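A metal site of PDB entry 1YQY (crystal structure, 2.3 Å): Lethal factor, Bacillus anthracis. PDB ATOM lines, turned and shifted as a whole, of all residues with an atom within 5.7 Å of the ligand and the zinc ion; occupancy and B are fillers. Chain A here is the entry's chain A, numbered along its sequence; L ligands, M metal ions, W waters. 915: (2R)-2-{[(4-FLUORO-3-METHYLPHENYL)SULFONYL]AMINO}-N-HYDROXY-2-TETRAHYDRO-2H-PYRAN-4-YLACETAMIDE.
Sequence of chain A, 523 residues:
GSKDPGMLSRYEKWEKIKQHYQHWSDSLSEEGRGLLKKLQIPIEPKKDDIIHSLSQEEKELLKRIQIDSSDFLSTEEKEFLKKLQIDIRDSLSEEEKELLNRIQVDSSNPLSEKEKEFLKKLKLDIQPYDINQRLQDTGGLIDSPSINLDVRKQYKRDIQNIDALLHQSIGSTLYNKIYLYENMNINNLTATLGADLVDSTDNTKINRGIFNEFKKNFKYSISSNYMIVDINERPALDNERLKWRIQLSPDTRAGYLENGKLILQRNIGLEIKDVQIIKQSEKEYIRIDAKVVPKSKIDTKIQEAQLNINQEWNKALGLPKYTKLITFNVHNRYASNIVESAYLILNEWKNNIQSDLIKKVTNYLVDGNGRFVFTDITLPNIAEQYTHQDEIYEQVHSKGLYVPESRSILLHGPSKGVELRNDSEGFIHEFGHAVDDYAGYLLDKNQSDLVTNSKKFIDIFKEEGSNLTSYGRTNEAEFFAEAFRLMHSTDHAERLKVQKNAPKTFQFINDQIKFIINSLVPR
OE1 of Glu 430 lies close to N19 of the ligand, at 3.4 Å.
An oxygen (O22) of the ligand sits at hydrogen-bond distance from the backbone NH (N) of Gly 400 (3.1 Å).
O of Gly 400 lies within hydrogen-bond range of N19 of the ligand, 2.8 Å away.
A nitrogen (N16) of the ligand is in hydrogen-bond range of the side-chain hydroxyl (OH) of Tyr 471.
OG of Ser 398 lies close to O22 of the ligand (3.4 Å).
The backbone NH of Lys 399 is in hydrogen-bond range of an oxygen (O22) of the ligand (3.2 Å).
ND1 of His 429 lies within hydrogen-bond range of OE2 of Glu 482.
OH of Tyr 471 sits close to OE1 of Glu 478 (3.4 Å).
N of Leu 401 lies close to OE1 of Glu 430 (3.4 Å).
The side-chain carboxylate (OE2) of Glu 430 sits at hydrogen-bond distance from the backbone NH (N) of Tyr 402, at 3.5 Å.
O of Gly 400 is in hydrogen-bond range of OG of Ser 398.
The side-chain carboxylate (OD2) of Asp 71 sits at hydrogen-bond distance from the side-chain hydroxyl (OH) of Tyr 471, 3.1 Å away.
The side-chain carboxylate of Glu 482 lies within salt-bridge range of the guanidinium group of Arg 485, 2.6 Å away.
Asp 71 touches the ligand.
Val 396 touches the ligand.
Leu 401 touches the ligand.
O of Val 418 touches C11 of the ligand (3.5 Å).
Leu 420 touches the ligand.
Gly 426 touches the ligand (CA to F10, 3.96 Å).
Glu 482 touches the ligand.
Arg 485 touches the ligand.
Hydrophobic or aromatic side chains that line the ligand: Val 396, Leu 401, Val 418, Leu 420, His 429, His 433 and Tyr 471.
Within 4 Å of the ligand: Asp 71, Val 396, Ser 398, Lys 399, Gly 400, Leu 401, Val 418, Leu 420, Gly 426, His 429, Glu 430, His 433, Tyr 471, Glu 478, Glu 482 and Arg 485.
The nearest printed residue that does not touch the zinc ion is Glu 430 (4.2 Å).
The zinc ion is bound by NE2 of His 433 (2.0 Å), NE2 of His 429 (2.1 Å), O21 of the ligand (2.2 Å), OE1 of Glu 478 (2.3 Å) and O20 of the ligand (2.4 Å).
Water W2 lies within hydrogen-bond range of the backbone NH (N) of Tyr 402 (3.3 Å) and a nitrogen (N19) of the ligand (3.4 Å).
Water W1 lies within hydrogen-bond range of O23 of the ligand, N of Lys 399 and O of Lys 416.
Water W3 lies within hydrogen-bond range of O of Val 418, OE1 of Glu 482 and NH2 of Arg 485.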
ATOM      1  N   ASP A  71      -6.201  19.635  19.088  1.00  0.00           N
ATOM      2  CA  ASP A  71      -5.431  19.152  17.946  1.00  0.00           C
ATOM      3  C   ASP A  71      -6.303  18.404  16.929  1.00  0.00           C
ATOM      4  O   ASP A  71      -5.789  17.761  15.993  1.00  0.00           O
ATOM      5  CB  ASP A  71      -4.297  18.215  18.421  1.00  0.00           C
ATOM      6  CG  ASP A  71      -4.764  17.213  19.456  1.00  0.00           C
ATOM      7  OD1 ASP A  71      -5.947  17.298  19.880  1.00  0.00           O
ATOM      8  OD2 ASP A  71      -3.949  16.341  19.851  1.00  0.00           O
ATOM      9  N   PHE A  72      -7.622  18.499  17.135  1.00  0.00           N
ATOM     10  CA  PHE A  72      -8.591  17.805  16.297  1.00  0.00           C
ATOM     11  C   PHE A  72      -9.629  18.740  15.616  1.00  0.00           C
ATOM     12  O   PHE A  72     -10.668  18.298  15.144  1.00  0.00           O
ATOM     13  CB  PHE A  72      -9.278  16.717  17.111  1.00  0.00           C
ATOM     14  CG  PHE A  72      -9.882  17.185  18.419  1.00  0.00           C
ATOM     15  CD1 PHE A  72     -11.222  17.541  18.496  1.00  0.00           C
ATOM     16  CD2 PHE A  72      -9.110  17.203  19.588  1.00  0.00           C
ATOM     17  CE1 PHE A  72     -11.793  17.891  19.714  1.00  0.00           C
ATOM     18  CE2 PHE A  72      -9.710  17.511  20.805  1.00  0.00           C
ATOM     19  CZ  PHE A  72     -11.033  17.891  20.872  1.00  0.00           C
ATOM     20  N   VAL A 396     -11.440  11.252  14.460  1.00  0.00           N
ATOM     21  CA  VAL A 396     -10.542  12.384  14.457  1.00  0.00           C
ATOM     22  C   VAL A 396      -9.979  12.691  13.099  1.00  0.00           C
ATOM     23  O   VAL A 396      -9.702  11.789  12.315  1.00  0.00           O
ATOM     24  CB  VAL A 396      -9.312  12.104  15.404  1.00  0.00           C
ATOM     25  CG1 VAL A 396      -8.290  13.094  15.202  1.00  0.00           C
ATOM     26  CG2 VAL A 396      -9.719  12.097  16.857  1.00  0.00           C
ATOM     27  N   HIS A 397      -9.836  13.981  12.801  1.00  0.00           N
ATOM     28  CA  HIS A 397      -9.142  14.394  11.580  1.00  0.00           C
ATOM     29  C   HIS A 397      -7.906  15.147  12.085  1.00  0.00           C
ATOM     30  O   HIS A 397      -8.014  15.913  13.034  1.00  0.00           O
ATOM     31  CB  HIS A 397      -9.968  15.290  10.681  1.00  0.00           C
ATOM     32  CG  HIS A 397      -9.169  15.884   9.564  1.00  0.00           C
ATOM     33  ND1 HIS A 397      -8.292  15.152   8.783  1.00  0.00           N
ATOM     34  CD2 HIS A 397      -9.025  17.177   9.163  1.00  0.00           C
ATOM     35  CE1 HIS A 397      -7.695  15.948   7.913  1.00  0.00           C
ATOM     36  NE2 HIS A 397      -8.108  17.183   8.128  1.00  0.00           N
ATOM     37  N   SER A 398      -6.738  14.852  11.529  1.00  0.00           N
ATOM     38  CA  SER A 398      -5.519  15.500  11.975  1.00  0.00           C
ATOM     39  C   SER A 398      -4.464  15.164  10.941  1.00  0.00           C
ATOM     40  O   SER A 398      -4.773  14.465   9.977  1.00  0.00           O
ATOM     41  CB  SER A 398      -5.097  14.974  13.366  1.00  0.00           C
ATOM     42  OG  SER A 398      -5.006  13.533  13.396  1.00  0.00           O
ATOM     43  N   LYS A 399      -3.248  15.685  11.123  1.00  0.00           N
ATOM     44  CA  LYS A 399      -2.138  15.400  10.216  1.00  0.00           C
ATOM     45  C   LYS A 399      -1.880  13.913  10.121  1.00  0.00           C
ATOM     46  O   LYS A 399      -1.641  13.375   9.035  1.00  0.00           O
ATOM     47  CB  LYS A 399      -0.830  16.058  10.724  1.00  0.00           C
ATOM     48  CG  LYS A 399       0.414  15.837   9.819  1.00  0.00           C
ATOM     49  CD  LYS A 399       0.044  16.230   8.398  1.00  0.00           C
ATOM     50  CE  LYS A 399       1.141  16.864   7.632  1.00  0.00           C
ATOM     51  NZ  LYS A 399       0.657  17.266   6.268  1.00  0.00           N
ATOM     52  N   GLY A 400      -1.809  13.257  11.275  1.00  0.00           N
ATOM     53  CA  GLY A 400      -1.448  11.844  11.302  1.00  0.00           C
ATOM     54  C   GLY A 400      -2.242  11.079  12.342  1.00  0.00           C
ATOM     55  O   GLY A 400      -2.784  11.680  13.277  1.00  0.00           O
ATOM     56  N   LEU A 401      -2.270   9.762  12.178  1.00  0.00           N
ATOM     57  CA  LEU A 401      -2.926   8.878  13.134  1.00  0.00           C
ATOM     58  C   LEU A 401      -2.396   7.441  13.066  1.00  0.00           C
ATOM     59  O   LEU A 401      -2.100   6.922  11.979  1.00  0.00           O
ATOM     60  CB  LEU A 401      -4.459   8.889  12.881  1.00  0.00           C
ATOM     61  CG  LEU A 401      -5.400   8.408  13.979  1.00  0.00           C
ATOM     62  CD1 LEU A 401      -5.297   9.281  15.241  1.00  0.00           C
ATOM     63  CD2 LEU A 401      -6.799   8.422  13.481  1.00  0.00           C
ATOM     64  N   TYR A 402      -2.272   6.795  14.220  1.00  0.00           N
ATOM     65  CA  TYR A 402      -1.940   5.384  14.255  1.00  0.00           C
ATOM     66  C   TYR A 402      -3.177   4.700  14.876  1.00  0.00           C
ATOM     67  O   TYR A 402      -3.626   5.088  15.971  1.00  0.00           O
ATOM     68  CB  TYR A 402      -0.746   5.081  15.123  1.00  0.00           C
ATOM     69  CG  TYR A 402      -0.506   3.571  15.209  1.00  0.00           C
ATOM     70  CD1 TYR A 402      -0.111   2.845  14.090  1.00  0.00           C
ATOM     71  CD2 TYR A 402      -0.793   2.871  16.362  1.00  0.00           C
ATOM     72  CE1 TYR A 402       0.036   1.458  14.143  1.00  0.00           C
ATOM     73  CE2 TYR A 402      -0.581   1.502  16.442  1.00  0.00           C
ATOM     74  CZ  TYR A 402      -0.219   0.812  15.320  1.00  0.00           C
ATOM     75  OH  TYR A 402      -0.154  -0.518  15.363  1.00  0.00           O
ATOM     76  N   LYS A 416      -1.459  20.632   8.390  1.00  0.00           N
ATOM     77  CA  LYS A 416      -0.224  21.004   9.045  1.00  0.00           C
ATOM     78  C   LYS A 416      -0.212  20.334  10.415  1.00  0.00           C
ATOM     79  O   LYS A 416      -1.222  20.266  11.090  1.00  0.00           O
ATOM     80  CB  LYS A 416      -0.186  22.543   9.188  1.00  0.00           C
ATOM     81  CG  LYS A 416       1.133  23.098   9.696  1.00  0.00           C
ATOM     82  CD  LYS A 416       2.038  23.504   8.546  1.00  0.00           C
ATOM     83  CE  LYS A 416       3.470  23.737   9.025  1.00  0.00           C
ATOM     84  NZ  LYS A 416       4.326  24.309   7.942  1.00  0.00           N
ATOM     85  N   GLY A 417       0.920  19.738  10.761  1.00  0.00           N
ATOM     86  CA  GLY A 417       1.027  19.066  12.052  1.00  0.00           C
ATOM     87  C   GLY A 417       1.678  20.045  13.012  1.00  0.00           C
ATOM     88  O   GLY A 417       2.278  21.034  12.594  1.00  0.00           O
ATOM     89  N   VAL A 418       1.544  19.757  14.297  1.00  0.00           N
ATOM     90  CA  VAL A 418       2.095  20.601  15.361  1.00  0.00           C
ATOM     91  C   VAL A 418       3.630  20.616  15.378  1.00  0.00           C
ATOM     92  O   VAL A 418       4.276  19.630  15.780  1.00  0.00           O
ATOM     93  CB  VAL A 418       1.609  20.100  16.752  1.00  0.00           C
ATOM     94  CG1 VAL A 418       2.159  20.969  17.855  1.00  0.00           C
ATOM     95  CG2 VAL A 418       0.070  20.070  16.794  1.00  0.00           C
ATOM     96  N   LEU A 420       6.007  20.607  13.040  1.00  0.00           N
ATOM     97  CA  LEU A 420       6.690  19.638  12.207  1.00  0.00           C
ATOM     98  C   LEU A 420       7.318  20.412  11.061  1.00  0.00           C
ATOM     99  O   LEU A 420       6.811  21.413  10.642  1.00  0.00           O
ATOM    100  CB  LEU A 420       5.697  18.606  11.668  1.00  0.00           C
ATOM    101  CG  LEU A 420       5.054  17.619  12.637  1.00  0.00           C
ATOM    102  CD1 LEU A 420       4.273  16.555  11.843  1.00  0.00           C
ATOM    103  CD2 LEU A 420       6.080  16.976  13.528  1.00  0.00           C
ATOM    104  N   GLU A 425       8.471  13.707   9.051  1.00  0.00           N
ATOM    105  CA  GLU A 425       8.533  13.752  10.511  1.00  0.00           C
ATOM    106  C   GLU A 425       7.233  13.291  11.131  1.00  0.00           C
ATOM    107  O   GLU A 425       7.239  12.553  12.116  1.00  0.00           O
ATOM    108  CB  GLU A 425       8.931  15.141  10.984  1.00  0.00           C
ATOM    109  CG  GLU A 425      10.339  15.561  10.588  1.00  0.00           C
ATOM    110  CD  GLU A 425      10.798  16.792  11.352  1.00  0.00           C
ATOM    111  OE1 GLU A 425       9.968  17.733  11.526  1.00  0.00           O
ATOM    112  OE2 GLU A 425      11.962  16.790  11.823  1.00  0.00           O
ATOM    113  N   GLY A 426       6.113  13.656  10.511  1.00  0.00           N
ATOM    114  CA  GLY A 426       4.807  13.190  11.015  1.00  0.00           C
ATOM    115  C   GLY A 426       4.759  11.682  10.950  1.00  0.00           C
ATOM    116  O   GLY A 426       4.371  11.000  11.912  1.00  0.00           O
ATOM    117  N   HIS A 429       6.843   9.925  13.657  1.00  0.00           N
ATOM    118  CA  HIS A 429       6.092  10.037  14.900  1.00  0.00           C
ATOM    119  C   HIS A 429       5.012   8.982  14.909  1.00  0.00           C
ATOM    120  O   HIS A 429       4.861   8.289  15.897  1.00  0.00           O
ATOM    121  CB  HIS A 429       5.460  11.457  15.026  1.00  0.00           C
ATOM    122  CG  HIS A 429       4.333  11.536  16.016  1.00  0.00           C
ATOM    123  ND1 HIS A 429       4.411  12.292  17.161  1.00  0.00           N
ATOM    124  CD2 HIS A 429       3.078  11.021  15.986  1.00  0.00           C
ATOM    125  CE1 HIS A 429       3.262  12.216  17.817  1.00  0.00           C
ATOM    126  NE2 HIS A 429       2.424  11.487  17.109  1.00  0.00           N
ATOM    127  N   GLU A 430       4.313   8.785  13.789  1.00  0.00           N
ATOM    128  CA  GLU A 430       3.258   7.748  13.726  1.00  0.00           C
ATOM    129  C   GLU A 430       3.890   6.372  13.919  1.00  0.00           C
ATOM    130  O   GLU A 430       3.362   5.525  14.618  1.00  0.00           O
ATOM    131  CB  GLU A 430       2.512   7.783  12.382  1.00  0.00           C
ATOM    132  CG  GLU A 430       1.583   8.950  12.080  1.00  0.00           C
ATOM    133  CD  GLU A 430       0.948   9.600  13.310  1.00  0.00           C
ATOM    134  OE1 GLU A 430       0.824  10.814  13.270  1.00  0.00           O
ATOM    135  OE2 GLU A 430       0.451   8.918  14.230  1.00  0.00           O
ATOM    136  N   HIS A 433       4.269   5.323  17.345  1.00  0.00           N
ATOM    137  CA  HIS A 433       3.096   4.719  17.928  1.00  0.00           C
ATOM    138  C   HIS A 433       3.040   3.244  17.668  1.00  0.00           C
ATOM    139  O   HIS A 433       2.623   2.480  18.524  1.00  0.00           O
ATOM    140  CB  HIS A 433       1.747   5.396  17.421  1.00  0.00           C
ATOM    141  CG  HIS A 433       1.532   6.787  17.940  1.00  0.00           C
ATOM    142  ND1 HIS A 433       1.548   7.104  19.280  1.00  0.00           N
ATOM    143  CD2 HIS A 433       1.350   7.960  17.288  1.00  0.00           C
ATOM    144  CE1 HIS A 433       1.367   8.399  19.430  1.00  0.00           C
ATOM    145  NE2 HIS A 433       1.242   8.944  18.235  1.00  0.00           N
ATOM    146  N   TYR A 471       3.792  19.448  22.579  1.00  0.00           N
ATOM    147  CA  TYR A 471       2.934  18.345  22.159  1.00  0.00           C
ATOM    148  C   TYR A 471       3.281  17.029  22.873  1.00  0.00           C
ATOM    149  O   TYR A 471       2.407  16.188  23.129  1.00  0.00           O
ATOM    150  CB  TYR A 471       2.929  18.184  20.633  1.00  0.00           C
ATOM    151  CG  TYR A 471       1.822  17.291  20.149  1.00  0.00           C
ATOM    152  CD1 TYR A 471       0.493  17.707  20.227  1.00  0.00           C
ATOM    153  CD2 TYR A 471       2.079  15.960  19.805  1.00  0.00           C
ATOM    154  CE1 TYR A 471      -0.547  16.851  19.903  1.00  0.00           C
ATOM    155  CE2 TYR A 471       1.026  15.100  19.499  1.00  0.00           C
ATOM    156  CZ  TYR A 471      -0.278  15.558  19.542  1.00  0.00           C
ATOM    157  OH  TYR A 471      -1.319  14.717  19.271  1.00  0.00           O
ATOM    158  N   GLU A 478       1.787   9.955  23.313  1.00  0.00           N
ATOM    159  CA  GLU A 478       2.333  11.025  22.480  1.00  0.00           C
ATOM    160  C   GLU A 478       3.741  11.436  22.865  1.00  0.00           C
ATOM    161  O   GLU A 478       4.536  11.899  22.023  1.00  0.00           O
ATOM    162  CB  GLU A 478       1.451  12.276  22.567  1.00  0.00           C
ATOM    163  CG  GLU A 478      -0.014  11.988  22.338  1.00  0.00           C
ATOM    164  CD  GLU A 478      -0.267  11.494  20.933  1.00  0.00           C
ATOM    165  OE1 GLU A 478       0.485  11.906  20.027  1.00  0.00           O
ATOM    166  OE2 GLU A 478      -1.120  10.603  20.766  1.00  0.00           O
ATOM    167  N   ALA A 481       5.966   8.909  21.412  1.00  0.00           N
ATOM    168  CA  ALA A 481       6.007   9.072  19.956  1.00  0.00           C
ATOM    169  C   ALA A 481       6.871  10.266  19.552  1.00  0.00           C
ATOM    170  O   ALA A 481       7.602  10.213  18.569  1.00  0.00           O
ATOM    171  CB  ALA A 481       4.590   9.164  19.393  1.00  0.00           C
ATOM    172  N   GLU A 482       6.746  11.352  20.302  1.00  0.00           N
ATOM    173  CA  GLU A 482       7.535  12.591  20.078  1.00  0.00           C
ATOM    174  C   GLU A 482       9.039  12.398  20.367  1.00  0.00           C
ATOM    175  O   GLU A 482       9.907  12.837  19.613  1.00  0.00           O
ATOM    176  CB  GLU A 482       6.986  13.735  20.962  1.00  0.00           C
ATOM    177  CG  GLU A 482       5.792  14.491  20.348  1.00  0.00           C
ATOM    178  CD  GLU A 482       6.120  15.094  19.000  1.00  0.00           C
ATOM    179  OE1 GLU A 482       6.250  16.329  18.917  1.00  0.00           O
ATOM    180  OE2 GLU A 482       6.273  14.328  18.015  1.00  0.00           O
ATOM    181  N   ARG A 485      10.358  10.284  17.628  1.00  0.00           N
ATOM    182  CA  ARG A 485      10.542  11.079  16.422  1.00  0.00           C
ATOM    183  C   ARG A 485      11.814  11.894  16.492  1.00  0.00           C
ATOM    184  O   ARG A 485      12.540  12.027  15.490  1.00  0.00           O
ATOM    185  CB  ARG A 485       9.387  12.068  16.265  1.00  0.00           C
ATOM    186  CG  ARG A 485       9.661  13.130  15.223  1.00  0.00           C
ATOM    187  CD  ARG A 485       8.401  13.946  14.904  1.00  0.00           C
ATOM    188  NE  ARG A 485       8.023  14.846  15.983  1.00  0.00           N
ATOM    189  CZ  ARG A 485       8.534  16.080  16.165  1.00  0.00           C
ATOM    190  NH1 ARG A 485       9.484  16.544  15.351  1.00  0.00           N
ATOM    191  NH2 ARG A 485       8.045  16.878  17.138  1.00  0.00           N
HETATM  192  C1  915 L   1       0.424  15.143  14.972  1.00  0.00           C
HETATM  193  C2  915 L   1       1.331  15.843  15.835  1.00  0.00           C
HETATM  194  C3  915 L   1       2.706  15.519  15.800  1.00  0.00           C
HETATM  195  C4  915 L   1       3.125  14.505  14.909  1.00  0.00           C
HETATM  196  C5  915 L   1       2.215  13.765  14.067  1.00  0.00           C
HETATM  197  C6  915 L   1       0.872  14.108  14.100  1.00  0.00           C
HETATM  198  F10 915 L   1       4.431  14.207  14.822  1.00  0.00           F
HETATM  199  C11 915 L   1       3.698  16.270  16.657  1.00  0.00           C
HETATM  200  S15 915 L   1      -1.285  15.604  14.956  1.00  0.00           S
HETATM  201  N16 915 L   1      -2.021  14.963  16.391  1.00  0.00           N
HETATM  202  C17 915 L   1      -2.535  13.590  16.373  1.00  0.00           C
HETATM  203  C18 915 L   1      -1.440  12.522  16.602  1.00  0.00           C
HETATM  204  N19 915 L   1      -1.482  11.476  15.726  1.00  0.00           N
HETATM  205  O20 915 L   1      -0.551  10.461  15.873  1.00  0.00           O
HETATM  206  O21 915 L   1      -0.630  12.578  17.482  1.00  0.00           O
HETATM  207  O22 915 L   1      -1.965  14.853  13.964  1.00  0.00           O
HETATM  208  O23 915 L   1      -1.378  17.054  15.037  1.00  0.00           O
HETATM  209  C27 915 L   1      -3.633  13.290  17.400  1.00  0.00           C
HETATM  210  C29 915 L   1      -4.938  14.164  17.318  1.00  0.00           C
HETATM  211  C30 915 L   1      -5.999  13.828  18.363  1.00  0.00           C
HETATM  212  O31 915 L   1      -6.308  12.451  18.284  1.00  0.00           O
HETATM  213  C32 915 L   1      -5.196  11.560  18.496  1.00  0.00           C
HETATM  214  C33 915 L   1      -4.100  11.815  17.444  1.00  0.00           C
HETATM  215 ZN    ZN M   1       0.635  10.880  17.968  1.00  0.00          ZN
HETATM  216  O   HOH W   1      -3.141  18.255  12.857  1.00  0.00           O
HETATM  217  O   HOH W   2      -2.424   8.478  17.082  1.00  0.00           O
HETATM  218  O   HOH W   3       5.536  18.836  17.937  1.00  0.00           O
